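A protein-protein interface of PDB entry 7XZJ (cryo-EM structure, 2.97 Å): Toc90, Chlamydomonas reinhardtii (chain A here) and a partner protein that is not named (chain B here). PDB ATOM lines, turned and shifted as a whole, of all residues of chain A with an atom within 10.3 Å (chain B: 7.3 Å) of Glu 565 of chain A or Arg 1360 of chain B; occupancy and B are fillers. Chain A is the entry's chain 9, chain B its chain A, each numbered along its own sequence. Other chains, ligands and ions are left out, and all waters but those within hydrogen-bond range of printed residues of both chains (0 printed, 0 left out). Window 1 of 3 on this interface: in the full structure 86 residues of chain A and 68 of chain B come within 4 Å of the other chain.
The side-chain amide nitrogen (NE2) of Gln 1066 of chain B is in hydrogen-bond range of the backbone carbonyl oxygen (O) of Thr 564 of chain A (3.2 Å). OG1 of Thr 564 of chain A sits at hydrogen-bond distance from NH2 of Arg 1459 of chain B. OG1 of Thr 564 of chain A sits at hydrogen-bond distance from NZ of Lys 1463 of chain B, at 3.2 Å. O of Glu 565 of chain A sits at hydrogen-bond distance from NZ of Lys 1463 of chain B (3.0 Å). OD1 of Asp 566 of chain A is in salt-bridge range of NZ of Lys 1463 of chain B. The side-chain amide oxygen (OD1) of Asn 573 of chain A lies close to the side-chain amide oxygen (OE1) of Gln 1066 of chain B (3.3 Å).
O of Glu 567 of chain A lies within hydrogen-bond range of OG of Ser 571 of chain A, 2.9 Å away. OD1 of Asn 573 of chain A sits close to O of Ala 569 of chain A, at 3.5 Å. The backbone carbonyl oxygen (O) of Asn 1278 of chain B sits at hydrogen-bond distance from the guanidinium group (NH2) of Arg 1358 of chain B. O of Lys 1355 of chain B lies within hydrogen-bond range of NH2 of Arg 1360 of chain B, at 3.0 Å. The backbone carbonyl oxygen (O) of Arg 1357 of chain B is in hydrogen-bond range of the guanidinium group (NH1) of Arg 1360 of chain B (2.9 Å).
Glu 565 of chain A touches just these residues of chain B: Arg 1358, Arg 1360 and Lys 1463. Of the printed residues of chain B, Ala 569 of chain A touches Gln 1066 (3.7 Å). No residue of chain A comes within 4 Å of Leu 1279 of chain B. No residue of chain A comes within 4 Å of Lys 1355 of chain B. Gly 1356 of chain B touches none of the printed residues of chain A. Arg 1358 of chain B touches just these residues of chain A: Glu 565, Asp 566 and Glu 567. Arg 1360 of chain B touches just one residue of chain A: Glu 565. No residue of chain A comes within 4 Å of Ser 1361 of chain B. Gly 1454 of chain B touches none of the printed residues of chain A. Gly 1456 of chain B touches none of the printed residues of chain A. Of the printed residues of chain A, Lys 1463 of chain B touches Thr 564 (3.2 Å), Glu 565 (3.0 Å) and Asp 566 (3.7 Å). The nearest residue of chain B that does not touch Glu 565 of chain A is Arg 1459 of chain B (4.6 Å).
Among the printed residues, pairs that only touch across the chains: Thr 552 of chain A with Tyr 1280 of chain B (3.9 Å), Thr 552 of chain A with Gln 1281 of chain B (3.4 Å), Ala 557 of chain A with Gln 1066 of chain B (3.8 Å), Glu 562 of chain A with Lys 1070 of chain B (3.8 Å), Val 563 of chain A with Gln 1066 of chain B (3.6 Å), Val 563 of chain A with Lys 1070 of chain B (3.99 Å), Thr 564 of chain A with Leu 1069 of chain B (3.8 Å), Thr 564 of chain A with Lys 1070 of chain B (3.9 Å), Glu 565 of chain A with Arg 1358 of chain B (3.7 Å), Glu 565 of chain A with Arg 1360 of chain B (3.4 Å), Asp 566 of chain A with Leu 1069 of chain B (3.5 Å), Asp 566 of chain A with Arg 1358 of chain B (3.9 Å), Glu 567 of chain A with Arg 1358 of chain B (3.8 Å), Ala 569 of chain A with Gln 1066 of chain B (3.7 Å) and Glu 570 of chain A with Gln 1066 of chain B (3.9 Å).
Hydrophobic or aromatic side chains of chain A within 4 Å of the printed part of chain B: Ala 557, Val 563 and Ala 569. Along chain A the printed residues that touch a printed residue of chain B span positions 552 to 573. Of the 26 printed residues of chain B, 9 touch a printed residue of chain A. Hydrophobic or aromatic side chains of chain B that line the printed part of chain A: Leu 1069. Among the printed residues, 21 pairs touch across the chains. Among the printed residues, Asp or Glu carboxylates within 4 Å of a Lys or Arg side-chain nitrogen of the other chain: Asp 566 of chain A with Lys 1463 of chain B (3.7 Å).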
ATOM      1  N   THR A 552      34.989  -6.404  22.632  1.00  0.00           N
ATOM      2  CA  THR A 552      36.011  -5.720  21.793  1.00  0.00           C
ATOM      3  C   THR A 552      36.201  -4.271  22.253  1.00  0.00           C
ATOM      4  O   THR A 552      35.185  -3.596  22.505  1.00  0.00           O
ATOM      5  CB  THR A 552      35.645  -5.814  20.306  1.00  0.00           C
ATOM      6  OG1 THR A 552      35.384  -7.188  20.023  1.00  0.00           O
ATOM      7  CG2 THR A 552      36.734  -5.304  19.389  1.00  0.00           C
ATOM      8  N   GLU A 554      37.216  -1.774  20.516  1.00  0.00           N
ATOM      9  CA  GLU A 554      36.572  -0.982  19.424  1.00  0.00           C
ATOM     10  C   GLU A 554      37.505   0.139  18.943  1.00  0.00           C
ATOM     11  O   GLU A 554      37.313   0.613  17.805  1.00  0.00           O
ATOM     12  CB  GLU A 554      35.149  -0.543  19.799  1.00  0.00           C
ATOM     13  CG  GLU A 554      34.358   0.088  18.668  1.00  0.00           C
ATOM     14  CD  GLU A 554      34.348   1.607  18.669  1.00  0.00           C
ATOM     15  OE1 GLU A 554      34.850   2.199  19.645  1.00  0.00           O
ATOM     16  OE2 GLU A 554      33.841   2.194  17.693  1.00  0.00           O
ATOM     17  N   ALA A 557      39.426  -2.023  16.592  1.00  0.00           N
ATOM     18  CA  ALA A 557      38.563  -2.808  15.680  1.00  0.00           C
ATOM     19  C   ALA A 557      38.609  -2.273  14.248  1.00  0.00           C
ATOM     20  O   ALA A 557      38.706  -3.092  13.315  1.00  0.00           O
ATOM     21  CB  ALA A 557      37.155  -2.815  16.217  1.00  0.00           C
ATOM     22  N   GLU A 561      38.448   3.889  13.085  1.00  0.00           N
ATOM     23  CA  GLU A 561      37.430   4.242  12.059  1.00  0.00           C
ATOM     24  C   GLU A 561      36.060   3.726  12.513  1.00  0.00           C
ATOM     25  O   GLU A 561      36.030   2.843  13.391  1.00  0.00           O
ATOM     26  CB  GLU A 561      37.828   3.687  10.692  1.00  0.00           C
ATOM     27  N   GLU A 562      34.976   4.248  11.926  1.00  0.00           N
ATOM     28  CA  GLU A 562      33.597   3.825  12.297  1.00  0.00           C
ATOM     29  C   GLU A 562      33.416   2.337  11.983  1.00  0.00           C
ATOM     30  O   GLU A 562      33.805   1.921  10.875  1.00  0.00           O
ATOM     31  CB  GLU A 562      32.563   4.666  11.545  1.00  0.00           C
ATOM     32  N   VAL A 563      32.834   1.575  12.915  1.00  0.00           N
ATOM     33  CA  VAL A 563      32.691   0.100  12.721  1.00  0.00           C
ATOM     34  C   VAL A 563      31.259  -0.328  13.052  1.00  0.00           C
ATOM     35  O   VAL A 563      30.598   0.381  13.836  1.00  0.00           O
ATOM     36  CB  VAL A 563      33.709  -0.675  13.580  1.00  0.00           C
ATOM     37  CG1 VAL A 563      35.124  -0.543  13.046  1.00  0.00           C
ATOM     38  CG2 VAL A 563      33.649  -0.265  15.043  1.00  0.00           C
ATOM     39  N   THR A 564      30.796  -1.435  12.463  1.00  0.00           N
ATOM     40  CA  THR A 564      29.446  -1.973  12.782  1.00  0.00           C
ATOM     41  C   THR A 564      29.623  -3.146  13.753  1.00  0.00           C
ATOM     42  O   THR A 564      30.788  -3.522  13.998  1.00  0.00           O
ATOM     43  CB  THR A 564      28.714  -2.392  11.501  1.00  0.00           C
ATOM     44  OG1 THR A 564      27.431  -2.908  11.852  1.00  0.00           O
ATOM     45  CG2 THR A 564      29.480  -3.420  10.699  1.00  0.00           C
ATOM     46  N   GLU A 565      28.530  -3.699  14.290  1.00  0.00           N
ATOM     47  CA  GLU A 565      28.675  -4.773  15.306  1.00  0.00           C
ATOM     48  C   GLU A 565      28.481  -6.145  14.658  1.00  0.00           C
ATOM     49  O   GLU A 565      27.339  -6.447  14.262  1.00  0.00           O
ATOM     50  CB  GLU A 565      27.655  -4.579  16.427  1.00  0.00           C
ATOM     51  N   ASP A 566      29.550  -6.942  14.567  1.00  0.00           N
ATOM     52  CA  ASP A 566      29.424  -8.330  14.048  1.00  0.00           C
ATOM     53  C   ASP A 566      30.149  -9.277  15.009  1.00  0.00           C
ATOM     54  O   ASP A 566      31.319  -9.002  15.334  1.00  0.00           O
ATOM     55  CB  ASP A 566      29.928  -8.451  12.609  1.00  0.00           C
ATOM     56  CG  ASP A 566      28.807  -8.474  11.582  1.00  0.00           C
ATOM     57  OD1 ASP A 566      27.638  -8.594  11.998  1.00  0.00           O
ATOM     58  OD2 ASP A 566      29.112  -8.372  10.379  1.00  0.00           O
ATOM     59  N   GLU A 567      29.477 -10.347  15.437  1.00  0.00           N
ATOM     60  CA  GLU A 567      30.097 -11.323  16.372  1.00  0.00           C
ATOM     61  C   GLU A 567      31.290 -11.992  15.684  1.00  0.00           C
ATOM     62  O   GLU A 567      32.327 -12.171  16.347  1.00  0.00           O
ATOM     63  CB  GLU A 567      29.062 -12.346  16.842  1.00  0.00           C
ATOM     64  CG  GLU A 567      28.107 -12.792  15.750  1.00  0.00           C
ATOM     65  CD  GLU A 567      27.095 -13.835  16.191  1.00  0.00           C
ATOM     66  OE1 GLU A 567      27.150 -14.248  17.365  1.00  0.00           O
ATOM     67  OE2 GLU A 567      26.255 -14.229  15.358  1.00  0.00           O
ATOM     68  N   GLY A 568      31.143 -12.331  14.401  1.00  0.00           N
ATOM     69  CA  GLY A 568      32.225 -13.012  13.665  1.00  0.00           C
ATOM     70  C   GLY A 568      33.459 -12.141  13.554  1.00  0.00           C
ATOM     71  O   GLY A 568      34.563 -12.664  13.788  1.00  0.00           O
ATOM     72  N   ALA A 569      33.284 -10.860  13.223  1.00  0.00           N
ATOM     73  CA  ALA A 569      34.448  -9.975  13.010  1.00  0.00           C
ATOM     74  C   ALA A 569      35.203  -9.835  14.332  1.00  0.00           C
ATOM     75  O   ALA A 569      36.438  -9.954  14.321  1.00  0.00           O
ATOM     76  CB  ALA A 569      33.984  -8.639  12.499  1.00  0.00           C
ATOM     77  N   GLU A 570      34.475  -9.617  15.427  1.00  0.00           N
ATOM     78  CA  GLU A 570      35.110  -9.432  16.754  1.00  0.00           C
ATOM     79  C   GLU A 570      35.931 -10.677  17.092  1.00  0.00           C
ATOM     80  O   GLU A 570      37.145 -10.541  17.336  1.00  0.00           O
ATOM     81  CB  GLU A 570      34.026  -9.204  17.805  1.00  0.00           C
ATOM     82  N   SER A 571      35.285 -11.845  17.080  1.00  0.00           N
ATOM     83  CA  SER A 571      35.980 -13.120  17.394  1.00  0.00           C
ATOM     84  C   SER A 571      37.206 -13.272  16.492  1.00  0.00           C
ATOM     85  O   SER A 571      38.294 -13.581  17.020  1.00  0.00           O
ATOM     86  CB  SER A 571      35.040 -14.278  17.222  1.00  0.00           C
ATOM     87  OG  SER A 571      33.836 -14.059  17.941  1.00  0.00           O
ATOM     88  N   ASN A 573      38.976 -11.050  14.976  1.00  0.00           N
ATOM     89  CA  ASN A 573      40.044 -10.068  15.288  1.00  0.00           C
ATOM     90  C   ASN A 573      40.826 -10.554  16.508  1.00  0.00           C
ATOM     91  O   ASN A 573      42.060 -10.460  16.477  1.00  0.00           O
ATOM     92  CB  ASN A 573      39.489  -8.654  15.465  1.00  0.00           C
ATOM     93  CG  ASN A 573      39.030  -8.022  14.168  1.00  0.00           C
ATOM     94  OD1 ASN A 573      38.303  -7.031  14.180  1.00  0.00           O
ATOM     95  ND2 ASN A 573      39.443  -8.588  13.047  1.00  0.00           N
ATOM     96  N   GLN B1066      35.401  -4.691   9.921  1.00  0.00           N
ATOM     97  CA  GLN B1066      34.195  -4.013  10.463  1.00  0.00           C
ATOM     98  C   GLN B1066      33.965  -2.697   9.714  1.00  0.00           C
ATOM     99  O   GLN B1066      32.800  -2.400   9.394  1.00  0.00           O
ATOM    100  CB  GLN B1066      34.329  -3.837  11.975  1.00  0.00           C
ATOM    101  CG  GLN B1066      34.948  -5.041  12.669  1.00  0.00           C
ATOM    102  CD  GLN B1066      34.709  -5.040  14.158  1.00  0.00           C
ATOM    103  OE1 GLN B1066      35.265  -5.849  14.896  1.00  0.00           O
ATOM    104  NE2 GLN B1066      33.867  -4.125  14.612  1.00  0.00           N
ATOM    105  N   LEU B1069      32.467  -3.284   6.234  1.00  0.00           N
ATOM    106  CA  LEU B1069      31.027  -3.632   6.366  1.00  0.00           C
ATOM    107  C   LEU B1069      30.226  -2.371   6.702  1.00  0.00           C
ATOM    108  O   LEU B1069      29.116  -2.219   6.162  1.00  0.00           O
ATOM    109  CB  LEU B1069      30.870  -4.704   7.448  1.00  0.00           C
ATOM    110  CG  LEU B1069      31.351  -6.100   7.055  1.00  0.00           C
ATOM    111  CD1 LEU B1069      31.502  -6.989   8.279  1.00  0.00           C
ATOM    112  CD2 LEU B1069      30.410  -6.732   6.042  1.00  0.00           C
ATOM    113  N   LYS B1070      30.771  -1.507   7.565  1.00  0.00           N
ATOM    114  CA  LYS B1070      30.053  -0.272   7.979  1.00  0.00           C
ATOM    115  C   LYS B1070      29.837   0.621   6.753  1.00  0.00           C
ATOM    116  O   LYS B1070      28.724   1.157   6.600  1.00  0.00           O
ATOM    117  CB  LYS B1070      30.858   0.466   9.054  1.00  0.00           C
ATOM    118  CG  LYS B1070      30.181   1.694   9.646  1.00  0.00           C
ATOM    119  CD  LYS B1070      28.878   1.371  10.344  1.00  0.00           C
ATOM    120  CE  LYS B1070      28.109   2.608  10.757  1.00  0.00           C
ATOM    121  NZ  LYS B1070      27.759   3.447   9.586  1.00  0.00           N
ATOM    122  N   ASN B1278      22.623  -9.181  22.222  1.00  0.00           N
ATOM    123  CA  ASN B1278      23.383  -8.445  23.265  1.00  0.00           C
ATOM    124  C   ASN B1278      24.760  -8.084  22.707  1.00  0.00           C
ATOM    125  O   ASN B1278      25.421  -8.986  22.159  1.00  0.00           O
ATOM    126  CB  ASN B1278      23.502  -9.260  24.555  1.00  0.00           C
ATOM    127  CG  ASN B1278      24.087  -8.473  25.708  1.00  0.00           C
ATOM    128  OD1 ASN B1278      24.063  -7.244  25.706  1.00  0.00           O
ATOM    129  ND2 ASN B1278      24.603  -9.174  26.705  1.00  0.00           N
ATOM    130  N   LEU B1279      25.192  -6.830  22.878  1.00  0.00           N
ATOM    131  CA  LEU B1279      26.547  -6.409  22.424  1.00  0.00           C
ATOM    132  C   LEU B1279      27.271  -5.699  23.577  1.00  0.00           C
ATOM    133  O   LEU B1279      26.661  -4.799  24.185  1.00  0.00           O
ATOM    134  CB  LEU B1279      26.404  -5.491  21.206  1.00  0.00           C
ATOM    135  N   TYR B1280      28.514  -6.099  23.866  1.00  0.00           N
ATOM    136  CA  TYR B1280      29.297  -5.488  24.974  1.00  0.00           C
ATOM    137  C   TYR B1280      30.656  -5.010  24.451  1.00  0.00           C
ATOM    138  O   TYR B1280      31.283  -5.747  23.665  1.00  0.00           O
ATOM    139  CB  TYR B1280      29.464  -6.487  26.122  1.00  0.00           C
ATOM    140  N   GLN B1281      31.091  -3.817  24.868  1.00  0.00           N
ATOM    141  CA  GLN B1281      32.389  -3.255  24.399  1.00  0.00           C
ATOM    142  C   GLN B1281      33.349  -2.932  25.548  1.00  0.00           C
ATOM    143  O   GLN B1281      32.908  -2.294  26.521  1.00  0.00           O
ATOM    144  CB  GLN B1281      32.148  -2.004  23.551  1.00  0.00           C
ATOM    145  N   SER B1353      27.897  -2.024  25.204  1.00  0.00           N
ATOM    146  CA  SER B1353      28.230  -1.169  24.034  1.00  0.00           C
ATOM    147  C   SER B1353      27.265   0.018  23.965  1.00  0.00           C
ATOM    148  O   SER B1353      26.094  -0.159  24.354  1.00  0.00           O
ATOM    149  CB  SER B1353      28.199  -1.963  22.757  1.00  0.00           C
ATOM    150  OG  SER B1353      26.882  -2.409  22.476  1.00  0.00           O
ATOM    151  N   SER B1354      27.746   1.177  23.502  1.00  0.00           N
ATOM    152  CA  SER B1354      26.884   2.381  23.362  1.00  0.00           C
ATOM    153  C   SER B1354      25.510   1.970  22.826  1.00  0.00           C
ATOM    154  O   SER B1354      24.500   2.333  23.460  1.00  0.00           O
ATOM    155  CB  SER B1354      27.536   3.406  22.473  1.00  0.00           C
ATOM    156  OG  SER B1354      27.848   2.851  21.204  1.00  0.00           O
ATOM    157  N   LYS B1355      25.474   1.244  21.704  1.00  0.00           N
ATOM    158  CA  LYS B1355      24.183   0.733  21.172  1.00  0.00           C
ATOM    159  C   LYS B1355      24.062  -0.726  21.616  1.00  0.00           C
ATOM    160  O   LYS B1355      24.626  -1.594  20.928  1.00  0.00           O
ATOM    161  CB  LYS B1355      24.125   0.903  19.652  1.00  0.00           C
ATOM    162  N   GLY B1356      23.346  -0.986  22.713  1.00  0.00           N
ATOM    163  CA  GLY B1356      23.290  -2.356  23.265  1.00  0.00           C
ATOM    164  C   GLY B1356      22.692  -3.361  22.300  1.00  0.00           C
ATOM    165  O   GLY B1356      23.224  -4.485  22.224  1.00  0.00           O
ATOM    166  N   ARG B1357      21.623  -2.988  21.592  1.00  0.00           N
ATOM    167  CA  ARG B1357      20.949  -3.969  20.704  1.00  0.00           C
ATOM    168  C   ARG B1357      21.884  -4.319  19.546  1.00  0.00           C
ATOM    169  O   ARG B1357      22.412  -3.383  18.917  1.00  0.00           O
ATOM    170  CB  ARG B1357      19.628  -3.397  20.180  1.00  0.00           C
ATOM    171  N   ARG B1358      22.064  -5.612  19.269  1.00  0.00           N
ATOM    172  CA  ARG B1358      22.889  -6.037  18.108  1.00  0.00           C
ATOM    173  C   ARG B1358      22.188  -5.543  16.842  1.00  0.00           C
ATOM    174  O   ARG B1358      22.887  -5.068  15.926  1.00  0.00           O
ATOM    175  CB  ARG B1358      23.046  -7.560  18.103  1.00  0.00           C
ATOM    176  CG  ARG B1358      23.923  -8.099  16.982  1.00  0.00           C
ATOM    177  CD  ARG B1358      25.398  -7.820  17.204  1.00  0.00           C
ATOM    178  NE  ARG B1358      25.906  -8.493  18.391  1.00  0.00           N
ATOM    179  CZ  ARG B1358      27.182  -8.505  18.759  1.00  0.00           C
ATOM    180  NH1 ARG B1358      28.088  -7.882  18.027  1.00  0.00           N
ATOM    181  NH2 ARG B1358      27.546  -9.145  19.855  1.00  0.00           N
ATOM    182  N   TYR B1359      20.856  -5.636  16.813  1.00  0.00           N
ATOM    183  CA  TYR B1359      20.073  -5.191  15.631  1.00  0.00           C
ATOM    184  C   TYR B1359      19.842  -3.683  15.747  1.00  0.00           C
ATOM    185  O   TYR B1359      18.716  -3.277  16.090  1.00  0.00           O
ATOM    186  CB  TYR B1359      18.746  -5.951  15.558  1.00  0.00           C
ATOM    187  CG  TYR B1359      18.881  -7.451  15.473  1.00  0.00           C
ATOM    188  CD1 TYR B1359      19.103  -8.219  16.604  1.00  0.00           C
ATOM    189  CD2 TYR B1359      18.779  -8.107  14.259  1.00  0.00           C
ATOM    190  CE1 TYR B1359      19.231  -9.596  16.532  1.00  0.00           C
ATOM    191  CE2 TYR B1359      18.902  -9.483  14.167  1.00  0.00           C
ATOM    192  CZ  TYR B1359      19.128 -10.230  15.307  1.00  0.00           C
ATOM    193  OH  TYR B1359      19.248 -11.586  15.224  1.00  0.00           O
ATOM    194  N   ARG B1360      20.878  -2.887  15.471  1.00  0.00           N
ATOM    195  CA  ARG B1360      20.773  -1.411  15.620  1.00  0.00           C
ATOM    196  C   ARG B1360      19.738  -0.867  14.635  1.00  0.00           C
ATOM    197  O   ARG B1360      19.725  -1.327  13.478  1.00  0.00           O
ATOM    198  CB  ARG B1360      22.141  -0.759  15.404  1.00  0.00           C
ATOM    199  CG  ARG B1360      23.112  -0.949  16.559  1.00  0.00           C
ATOM    200  CD  ARG B1360      24.457  -1.484  16.109  1.00  0.00           C
ATOM    201  NE  ARG B1360      25.524  -1.197  17.057  1.00  0.00           N
ATOM    202  CZ  ARG B1360      25.860  -1.976  18.078  1.00  0.00           C
ATOM    203  NH1 ARG B1360      25.207  -3.103  18.298  1.00  0.00           N
ATOM    204  NH2 ARG B1360      26.847  -1.621  18.882  1.00  0.00           N
ATOM    205  N   SER B1361      18.911   0.083  15.082  1.00  0.00           N
ATOM    206  CA  SER B1361      17.883   0.698  14.203  1.00  0.00           C
ATOM    207  C   SER B1361      17.760   2.186  14.544  1.00  0.00           C
ATOM    208  O   SER B1361      17.674   2.506  15.745  1.00  0.00           O
ATOM    209  CB  SER B1361      16.556  -0.002  14.341  1.00  0.00           C
ATOM    210  OG  SER B1361      16.626  -1.331  13.848  1.00  0.00           O
ATOM    211  N   LEU B1362      17.750   3.054  13.529  1.00  0.00           N
ATOM    212  CA  LEU B1362      17.638   4.487  13.754  1.00  0.00           C
ATOM    213  C   LEU B1362      16.268   4.833  14.329  1.00  0.00           C
ATOM    214  O   LEU B1362      15.254   4.217  13.991  1.00  0.00           O
ATOM    215  CB  LEU B1362      17.866   5.253  12.449  1.00  0.00           C
ATOM    216  N   THR B1452      13.522  -5.361  19.124  1.00  0.00           N
ATOM    217  CA  THR B1452      14.462  -4.985  18.065  1.00  0.00           C
ATOM    218  C   THR B1452      13.802  -4.221  16.923  1.00  0.00           C
ATOM    219  O   THR B1452      14.446  -3.997  15.891  1.00  0.00           O
ATOM    220  CB  THR B1452      15.210  -6.192  17.485  1.00  0.00           C
ATOM    221  OG1 THR B1452      14.290  -7.041  16.787  1.00  0.00           O
ATOM    222  CG2 THR B1452      15.885  -6.986  18.588  1.00  0.00           C
ATOM    223  N   GLY B1454      11.980  -2.934  13.642  1.00  0.00           N
ATOM    224  CA  GLY B1454      12.097  -3.450  12.295  1.00  0.00           C
ATOM    225  C   GLY B1454      13.289  -2.848  11.583  1.00  0.00           C
ATOM    226  O   GLY B1454      13.751  -1.757  11.912  1.00  0.00           O
ATOM    227  N   ASN B1455      13.792  -3.596  10.602  1.00  0.00           N
ATOM    228  CA  ASN B1455      14.913  -3.295   9.716  1.00  0.00           C
ATOM    229  C   ASN B1455      16.270  -3.483  10.393  1.00  0.00           C
ATOM    230  O   ASN B1455      17.294  -3.430   9.709  1.00  0.00           O
ATOM    231  CB  ASN B1455      14.848  -1.879   9.114  1.00  0.00           C
ATOM    232  CG  ASN B1455      13.534  -1.604   8.412  1.00  0.00           C
ATOM    233  OD1 ASN B1455      12.950  -0.529   8.545  1.00  0.00           O
ATOM    234  ND2 ASN B1455      13.057  -2.587   7.658  1.00  0.00           N
ATOM    235  N   GLY B1456      16.313  -3.756  11.697  1.00  0.00           N
ATOM    236  CA  GLY B1456      17.555  -4.216  12.293  1.00  0.00           C
ATOM    237  C   GLY B1456      17.935  -5.591  11.777  1.00  0.00           C
ATOM    238  O   GLY B1456      19.111  -5.868  11.502  1.00  0.00           O
ATOM    239  N   LYS B1457      16.937  -6.463  11.619  1.00  0.00           N
ATOM    240  CA  LYS B1457      17.166  -7.737  10.956  1.00  0.00           C
ATOM    241  C   LYS B1457      17.647  -7.523   9.530  1.00  0.00           C
ATOM    242  O   LYS B1457      18.491  -8.276   9.038  1.00  0.00           O
ATOM    243  CB  LYS B1457      15.893  -8.580  10.967  1.00  0.00           C
ATOM    244  CG  LYS B1457      16.083  -9.963  10.372  1.00  0.00           C
ATOM    245  CD  LYS B1457      17.239 -10.680  11.052  1.00  0.00           C
ATOM    246  CE  LYS B1457      17.519 -12.028  10.410  1.00  0.00           C
ATOM    247  NZ  LYS B1457      16.377 -12.972  10.561  1.00  0.00           N
ATOM    248  N   ARG B1459      19.468  -4.968   8.463  1.00  0.00           N
ATOM    249  CA  ARG B1459      20.869  -4.568   8.553  1.00  0.00           C
ATOM    250  C   ARG B1459      21.772  -5.779   8.773  1.00  0.00           C
ATOM    251  O   ARG B1459      22.768  -5.971   8.054  1.00  0.00           O
ATOM    252  CB  ARG B1459      21.025  -3.555   9.690  1.00  0.00           C
ATOM    253  CG  ARG B1459      22.375  -2.864   9.793  1.00  0.00           C
ATOM    254  CD  ARG B1459      22.325  -1.783  10.873  1.00  0.00           C
ATOM    255  NE  ARG B1459      23.560  -1.018  10.995  1.00  0.00           N
ATOM    256  CZ  ARG B1459      24.520  -1.268  11.881  1.00  0.00           C
ATOM    257  NH1 ARG B1459      24.429  -2.273  12.736  1.00  0.00           N
ATOM    258  NH2 ARG B1459      25.597  -0.490  11.907  1.00  0.00           N
ATOM    259  N   VAL B1460      21.402  -6.639   9.724  1.00  0.00           N
ATOM    260  CA  VAL B1460      22.233  -7.801  10.028  1.00  0.00           C
ATOM    261  C   VAL B1460      22.264  -8.765   8.847  1.00  0.00           C
ATOM    262  O   VAL B1460      23.320  -9.310   8.494  1.00  0.00           O
ATOM    263  CB  VAL B1460      21.735  -8.484  11.314  1.00  0.00           C
ATOM    264  CG1 VAL B1460      22.488  -9.777  11.561  1.00  0.00           C
ATOM    265  CG2 VAL B1460      21.902  -7.546  12.495  1.00  0.00           C
ATOM    266  N   LYS B1463      24.578  -7.522   6.164  1.00  0.00           N
ATOM    267  CA  LYS B1463      25.963  -7.803   6.539  1.00  0.00           C
ATOM    268  C   LYS B1463      26.331  -9.256   6.251  1.00  0.00           C
ATOM    269  O   LYS B1463      27.391  -9.541   5.671  1.00  0.00           O
ATOM    270  CB  LYS B1463      26.187  -7.480   8.016  1.00  0.00           C
ATOM    271  CG  LYS B1463      26.338  -5.999   8.299  1.00  0.00           C
ATOM    272  CD  LYS B1463      26.603  -5.713   9.768  1.00  0.00           C
ATOM    273  CE  LYS B1463      25.359  -5.914  10.612  1.00  0.00           C
ATOM    274  NZ  LYS B1463      25.604  -5.531  12.028  1.00  0.00           N
ATOM    275  N   LYS B1464      25.454 -10.190   6.630  1.00  0.00           N
ATOM    276  CA  LYS B1464      25.756 -11.605   6.429  1.00  0.00           C
ATOM    277  C   LYS B1464      25.872 -11.951   4.946  1.00  0.00           C
ATOM    278  O   LYS B1464      26.791 -12.678   4.538  1.00  0.00           O
ATOM    279  CB  LYS B1464      24.687 -12.468   7.097  1.00  0.00           C
ATOM    280  CG  LYS B1464      24.539 -12.231   8.589  1.00  0.00           C
ATOM    281  CD  LYS B1464      25.830 -12.529   9.330  1.00  0.00           C
ATOM    282  CE  LYS B1464      25.668 -12.288  10.822  1.00  0.00           C
ATOM    283  NZ  LYS B1464      24.591 -13.133  11.413  1.00  0.00           N
